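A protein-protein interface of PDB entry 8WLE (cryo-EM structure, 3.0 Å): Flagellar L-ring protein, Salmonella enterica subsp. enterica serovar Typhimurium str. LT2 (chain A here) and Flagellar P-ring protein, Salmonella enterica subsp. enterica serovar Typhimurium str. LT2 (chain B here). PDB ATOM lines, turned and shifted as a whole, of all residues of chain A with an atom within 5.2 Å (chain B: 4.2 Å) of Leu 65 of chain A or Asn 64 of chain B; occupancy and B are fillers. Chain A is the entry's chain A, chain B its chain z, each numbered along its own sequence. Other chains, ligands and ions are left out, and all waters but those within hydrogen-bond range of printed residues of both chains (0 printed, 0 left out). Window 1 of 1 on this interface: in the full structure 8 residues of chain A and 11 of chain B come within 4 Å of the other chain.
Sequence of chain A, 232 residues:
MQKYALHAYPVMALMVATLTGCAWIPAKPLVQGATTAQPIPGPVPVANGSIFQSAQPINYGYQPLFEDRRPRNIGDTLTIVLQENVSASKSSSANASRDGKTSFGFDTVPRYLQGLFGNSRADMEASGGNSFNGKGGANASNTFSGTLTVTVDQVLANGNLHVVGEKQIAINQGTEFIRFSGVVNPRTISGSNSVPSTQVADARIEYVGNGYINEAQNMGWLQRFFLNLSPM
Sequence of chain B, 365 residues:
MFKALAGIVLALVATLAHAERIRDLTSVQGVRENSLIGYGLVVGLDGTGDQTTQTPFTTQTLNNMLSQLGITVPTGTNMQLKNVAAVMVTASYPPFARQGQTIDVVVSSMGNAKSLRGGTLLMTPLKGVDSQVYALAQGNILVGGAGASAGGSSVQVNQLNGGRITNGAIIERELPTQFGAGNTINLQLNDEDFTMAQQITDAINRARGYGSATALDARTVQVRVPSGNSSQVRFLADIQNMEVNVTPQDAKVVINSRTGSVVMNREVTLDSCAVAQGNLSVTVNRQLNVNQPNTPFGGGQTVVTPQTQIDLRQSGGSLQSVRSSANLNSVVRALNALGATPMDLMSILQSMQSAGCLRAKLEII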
ATOM      1  N   GLN A  63      20.565 -17.955  22.973  1.00  0.00           N
ATOM      2  CA  GLN A  63      20.902 -17.349  21.693  1.00  0.00           C
ATOM      3  C   GLN A  63      19.614 -16.885  21.030  1.00  0.00           C
ATOM      4  O   GLN A  63      18.718 -17.712  20.787  1.00  0.00           O
ATOM      5  CB  GLN A  63      21.642 -18.339  20.799  1.00  0.00           C
ATOM      6  CG  GLN A  63      22.975 -18.789  21.370  1.00  0.00           C
ATOM      7  CD  GLN A  63      23.381 -20.162  20.889  1.00  0.00           C
ATOM      8  OE1 GLN A  63      22.611 -21.118  20.982  1.00  0.00           O
ATOM      9  NE2 GLN A  63      24.596 -20.271  20.372  1.00  0.00           N
ATOM     10  N   PRO A  64      19.458 -15.597  20.736  1.00  0.00           N
ATOM     11  CA  PRO A  64      18.205 -15.130  20.127  1.00  0.00           C
ATOM     12  C   PRO A  64      17.997 -15.711  18.739  1.00  0.00           C
ATOM     13  O   PRO A  64      18.917 -16.292  18.158  1.00  0.00           O
ATOM     14  CB  PRO A  64      18.379 -13.607  20.082  1.00  0.00           C
ATOM     15  CG  PRO A  64      19.429 -13.313  21.099  1.00  0.00           C
ATOM     16  CD  PRO A  64      20.353 -14.483  21.073  1.00  0.00           C
ATOM     17  N   LEU A  65      16.803 -15.542  18.187  1.00  0.00           N
ATOM     18  CA  LEU A  65      16.449 -16.170  16.925  1.00  0.00           C
ATOM     19  C   LEU A  65      16.221 -15.182  15.797  1.00  0.00           C
ATOM     20  O   LEU A  65      16.496 -15.514  14.642  1.00  0.00           O
ATOM     21  CB  LEU A  65      15.189 -17.028  17.103  1.00  0.00           C
ATOM     22  CG  LEU A  65      15.015 -18.260  16.215  1.00  0.00           C
ATOM     23  CD1 LEU A  65      16.100 -19.283  16.494  1.00  0.00           C
ATOM     24  CD2 LEU A  65      13.640 -18.866  16.422  1.00  0.00           C
ATOM     25  N   PHE A  66      15.720 -13.986  16.094  1.00  0.00           N
ATOM     26  CA  PHE A  66      15.498 -12.960  15.091  1.00  0.00           C
ATOM     27  C   PHE A  66      16.428 -11.769  15.245  1.00  0.00           C
ATOM     28  O   PHE A  66      16.505 -10.942  14.330  1.00  0.00           O
ATOM     29  CB  PHE A  66      14.041 -12.480  15.137  1.00  0.00           C
ATOM     30  CG  PHE A  66      13.041 -13.595  15.129  1.00  0.00           C
ATOM     31  CD1 PHE A  66      12.779 -14.296  13.968  1.00  0.00           C
ATOM     32  CD2 PHE A  66      12.367 -13.946  16.282  1.00  0.00           C
ATOM     33  CE1 PHE A  66      11.863 -15.322  13.960  1.00  0.00           C
ATOM     34  CE2 PHE A  66      11.452 -14.968  16.275  1.00  0.00           C
ATOM     35  CZ  PHE A  66      11.199 -15.657  15.115  1.00  0.00           C
ATOM     36  N   GLU A  67      17.129 -11.659  16.368  1.00  0.00           N
ATOM     37  CA  GLU A  67      18.078 -10.578  16.561  1.00  0.00           C
ATOM     38  C   GLU A  67      19.311 -10.826  15.704  1.00  0.00           C
ATOM     39  O   GLU A  67      19.752 -11.967  15.542  1.00  0.00           O
ATOM     40  CB  GLU A  67      18.466 -10.460  18.034  1.00  0.00           C
ATOM     41  CG  GLU A  67      17.288 -10.324  18.983  1.00  0.00           C
ATOM     42  CD  GLU A  67      17.722 -10.092  20.415  1.00  0.00           C
ATOM     43  OE1 GLU A  67      18.783  -9.467  20.625  1.00  0.00           O
ATOM     44  OE2 GLU A  67      17.008 -10.542  21.338  1.00  0.00           O
ATOM     45  N   ASP A  68      19.859  -9.749  15.146  1.00  0.00           N
ATOM     46  CA  ASP A  68      21.023  -9.867  14.283  1.00  0.00           C
ATOM     47  C   ASP A  68      22.201 -10.441  15.059  1.00  0.00           C
ATOM     48  O   ASP A  68      22.302 -10.308  16.280  1.00  0.00           O
ATOM     49  CB  ASP A  68      21.396  -8.506  13.700  1.00  0.00           C
ATOM     50  CG  ASP A  68      20.325  -7.948  12.797  1.00  0.00           C
ATOM     51  OD1 ASP A  68      19.390  -8.700  12.447  1.00  0.00           O
ATOM     52  OD2 ASP A  68      20.409  -6.756  12.438  1.00  0.00           O
ATOM     53  N   ARG A  69      23.097 -11.101  14.330  1.00  0.00           N
ATOM     54  CA  ARG A  69      24.268 -11.712  14.947  1.00  0.00           C
ATOM     55  C   ARG A  69      25.268 -10.618  15.291  1.00  0.00           C
ATOM     56  O   ARG A  69      26.015 -10.140  14.435  1.00  0.00           O
ATOM     57  CB  ARG A  69      24.878 -12.762  14.027  1.00  0.00           C
ATOM     58  CG  ARG A  69      24.952 -12.369  12.570  1.00  0.00           C
ATOM     59  CD  ARG A  69      25.435 -13.541  11.735  1.00  0.00           C
ATOM     60  NE  ARG A  69      26.084 -13.100  10.509  1.00  0.00           N
ATOM     61  CZ  ARG A  69      27.386 -12.878  10.400  1.00  0.00           C
ATOM     62  NH1 ARG A  69      28.203 -13.047  11.426  1.00  0.00           N
ATOM     63  NH2 ARG A  69      27.877 -12.475   9.233  1.00  0.00           N
ATOM     64  N   GLY A 191      23.371  -5.850   9.815  1.00  0.00           N
ATOM     65  CA  GLY A 191      22.845  -7.202   9.877  1.00  0.00           C
ATOM     66  C   GLY A 191      23.847  -8.269   9.503  1.00  0.00           C
ATOM     67  O   GLY A 191      23.675  -9.429   9.892  1.00  0.00           O
ATOM     68  N   GLN B  60      14.896 -10.283   6.564  1.00  0.00           N
ATOM     69  CA  GLN B  60      16.162 -10.205   7.286  1.00  0.00           C
ATOM     70  C   GLN B  60      16.121 -11.045   8.556  1.00  0.00           C
ATOM     71  O   GLN B  60      17.057 -11.796   8.849  1.00  0.00           O
ATOM     72  CB  GLN B  60      16.487  -8.750   7.608  1.00  0.00           C
ATOM     73  CG  GLN B  60      17.775  -8.563   8.377  1.00  0.00           C
ATOM     74  CD  GLN B  60      18.086  -7.109   8.615  1.00  0.00           C
ATOM     75  OE1 GLN B  60      17.443  -6.227   8.049  1.00  0.00           O
ATOM     76  NE2 GLN B  60      19.075  -6.845   9.457  1.00  0.00           N
ATOM     77  N   THR B  61      15.029 -10.952   9.312  1.00  0.00           N
ATOM     78  CA  THR B  61      14.918 -11.720  10.542  1.00  0.00           C
ATOM     79  C   THR B  61      14.652 -13.194  10.275  1.00  0.00           C
ATOM     80  O   THR B  61      15.086 -14.044  11.059  1.00  0.00           O
ATOM     81  CB  THR B  61      13.825 -11.128  11.425  1.00  0.00           C
ATOM     82  OG1 THR B  61      12.608 -11.036  10.680  1.00  0.00           O
ATOM     83  CG2 THR B  61      14.232  -9.746  11.880  1.00  0.00           C
ATOM     84  N   LEU B  62      13.972 -13.527   9.176  1.00  0.00           N
ATOM     85  CA  LEU B  62      13.860 -14.933   8.803  1.00  0.00           C
ATOM     86  C   LEU B  62      15.227 -15.520   8.480  1.00  0.00           C
ATOM     87  O   LEU B  62      15.543 -16.645   8.886  1.00  0.00           O
ATOM     88  CB  LEU B  62      12.917 -15.094   7.615  1.00  0.00           C
ATOM     89  CG  LEU B  62      12.601 -16.551   7.273  1.00  0.00           C
ATOM     90  CD1 LEU B  62      11.352 -17.015   7.998  1.00  0.00           C
ATOM     91  CD2 LEU B  62      12.471 -16.755   5.776  1.00  0.00           C
ATOM     92  N   ASN B  63      16.055 -14.770   7.747  1.00  0.00           N
ATOM     93  CA  ASN B  63      17.408 -15.233   7.459  1.00  0.00           C
ATOM     94  C   ASN B  63      18.232 -15.341   8.733  1.00  0.00           C
ATOM     95  O   ASN B  63      19.057 -16.248   8.866  1.00  0.00           O
ATOM     96  CB  ASN B  63      18.085 -14.301   6.459  1.00  0.00           C
ATOM     97  CG  ASN B  63      17.495 -14.413   5.070  1.00  0.00           C
ATOM     98  OD1 ASN B  63      17.205 -13.408   4.422  1.00  0.00           O
ATOM     99  ND2 ASN B  63      17.315 -15.641   4.603  1.00  0.00           N
ATOM    100  N   ASN B  64      18.036 -14.417   9.673  1.00  0.00           N
ATOM    101  CA  ASN B  64      18.701 -14.525  10.968  1.00  0.00           C
ATOM    102  C   ASN B  64      18.299 -15.806  11.687  1.00  0.00           C
ATOM    103  O   ASN B  64      19.145 -16.509  12.251  1.00  0.00           O
ATOM    104  CB  ASN B  64      18.380 -13.306  11.831  1.00  0.00           C
ATOM    105  CG  ASN B  64      19.121 -12.070  11.388  1.00  0.00           C
ATOM    106  OD1 ASN B  64      20.189 -12.156  10.787  1.00  0.00           O
ATOM    107  ND2 ASN B  64      18.560 -10.906  11.690  1.00  0.00           N
ATOM    108  N   MET B  65      17.004 -16.122  11.683  1.00  0.00           N
ATOM    109  CA  MET B  65      16.539 -17.336  12.343  1.00  0.00           C
ATOM    110  C   MET B  65      17.130 -18.575  11.685  1.00  0.00           C
ATOM    111  O   MET B  65      17.562 -19.508  12.368  1.00  0.00           O
ATOM    112  CB  MET B  65      15.015 -17.400  12.321  1.00  0.00           C
ATOM    113  CG  MET B  65      14.465 -18.662  12.951  1.00  0.00           C
ATOM    114  SD  MET B  65      12.676 -18.769  12.846  1.00  0.00           S
ATOM    115  CE  MET B  65      12.444 -18.704  11.074  1.00  0.00           C
ATOM    116  N   LEU B  66      17.153 -18.603  10.353  1.00  0.00           N
ATOM    117  CA  LEU B  66      17.728 -19.746   9.654  1.00  0.00           C
ATOM    118  C   LEU B  66      19.218 -19.874   9.936  1.00  0.00           C
ATOM    119  O   LEU B  66      19.725 -20.982  10.139  1.00  0.00           O
ATOM    120  CB  LEU B  66      17.479 -19.630   8.152  1.00  0.00           C
ATOM    121  CG  LEU B  66      16.023 -19.644   7.700  1.00  0.00           C
ATOM    122  CD1 LEU B  66      15.950 -19.647   6.190  1.00  0.00           C
ATOM    123  CD2 LEU B  66      15.296 -20.837   8.276  1.00  0.00           C
ATOM    124  N   SER B  67      19.940 -18.751   9.945  1.00  0.00           N
ATOM    125  CA  SER B  67      21.368 -18.783  10.233  1.00  0.00           C
ATOM    126  C   SER B  67      21.628 -19.296  11.640  1.00  0.00           C
ATOM    127  O   SER B  67      22.586 -20.040  11.872  1.00  0.00           O
ATOM    128  CB  SER B  67      21.968 -17.393  10.047  1.00  0.00           C
ATOM    129  OG  SER B  67      23.353 -17.393  10.338  1.00  0.00           O
ATOM    130  N   GLN B  68      20.790 -18.898  12.596  1.00  0.00           N
ATOM    131  CA  GLN B  68      20.900 -19.440  13.943  1.00  0.00           C
ATOM    132  C   GLN B  68      20.619 -20.935  13.959  1.00  0.00           C
ATOM    133  O   GLN B  68      21.297 -21.694  14.660  1.00  0.00           O
ATOM    134  CB  GLN B  68      19.950 -18.707  14.884  1.00  0.00           C
ATOM    135  CG  GLN B  68      20.018 -19.197  16.309  1.00  0.00           C
ATOM    136  CD  GLN B  68      21.397 -19.033  16.902  1.00  0.00           C
ATOM    137  OE1 GLN B  68      21.998 -17.965  16.813  1.00  0.00           O
ATOM    138  NE2 GLN B  68      21.910 -20.097  17.504  1.00  0.00           N
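The backbone carbonyl oxygen (O) of Leu 65 of chain A sits close to the backbone NH (N) of Met 65 of chain B. The backbone carbonyl oxygen of Phe 66 of chain A lies within hydrogen-bond range of the side-chain amide nitrogen of Asn 64 of chain B (3.3 Å). OD2 of Asp 68 of chain A sits at hydrogen-bond distance from NE2 of Gln 60 of chain B, 3.3 Å away. The side-chain carboxylate of Asp 68 of chain A is in hydrogen-bond range of the side-chain amide nitrogen of Asn 64 of chain B (2.5 Å).
The backbone carbonyl oxygen (O) of Gln 60 of chain B lies close to the side-chain amide nitrogen (ND2) of Asn 64 of chain B, 3.3 Å away.
CD of Gln 63 of chain A touches NE2 of Gln 68 of chain B (3.7 Å). CG of Gln 68 of chain B touches O of Pro 64 of chain A, at 3.6 Å. Asn 64 of chain B touches Leu 65 of chain A. CD1 of Leu 65 of chain A touches CG of Gln 68 of chain B, 3.9 Å away. Phe 66 of chain A touches Thr 61 of chain B (O to CG2, 3.5 Å). Met 65 of chain B touches Phe 66 of chain A. Gln 60 of chain B touches Gly 191 of chain A (NE2 to CA, 3.8 Å).
Leu 65 of chain A touches three residues of chain B. Asn 64 of chain B touches just these residues of chain A: Leu 65 (3.5 Å), Phe 66 (3.3 Å) and Asp 68 (2.5 Å). Of the printed residues of chain A, Met 65 of chain B touches Leu 65 (2.9 Å) and Phe 66 (3.7 Å). Printed residues of chain B within 4 Å of Gly 191 of chain A: Gln 60. Of the printed residues of chain A, Thr 61 of chain B touches Phe 66. Glu 67 of chain A touches none of the printed residues of chain B. Asn 63 of chain B touches none of the printed residues of chain A. The nearest residue of chain B that does not touch Leu 65 of chain A is Thr 61 of chain B (4.1 Å). The nearest residue of chain A that does not touch Asn 64 of chain B is Glu 67 of chain A (4.1 Å).
Along chain B the printed residues that touch a printed residue of chain A span positions 60 to 68. Among the printed residues, 11 pairs touch across the chains. Among the printed residues, no Asp or Glu carboxylate lies within 4 Å of a Lys or Arg side-chain nitrogen of the other chain.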
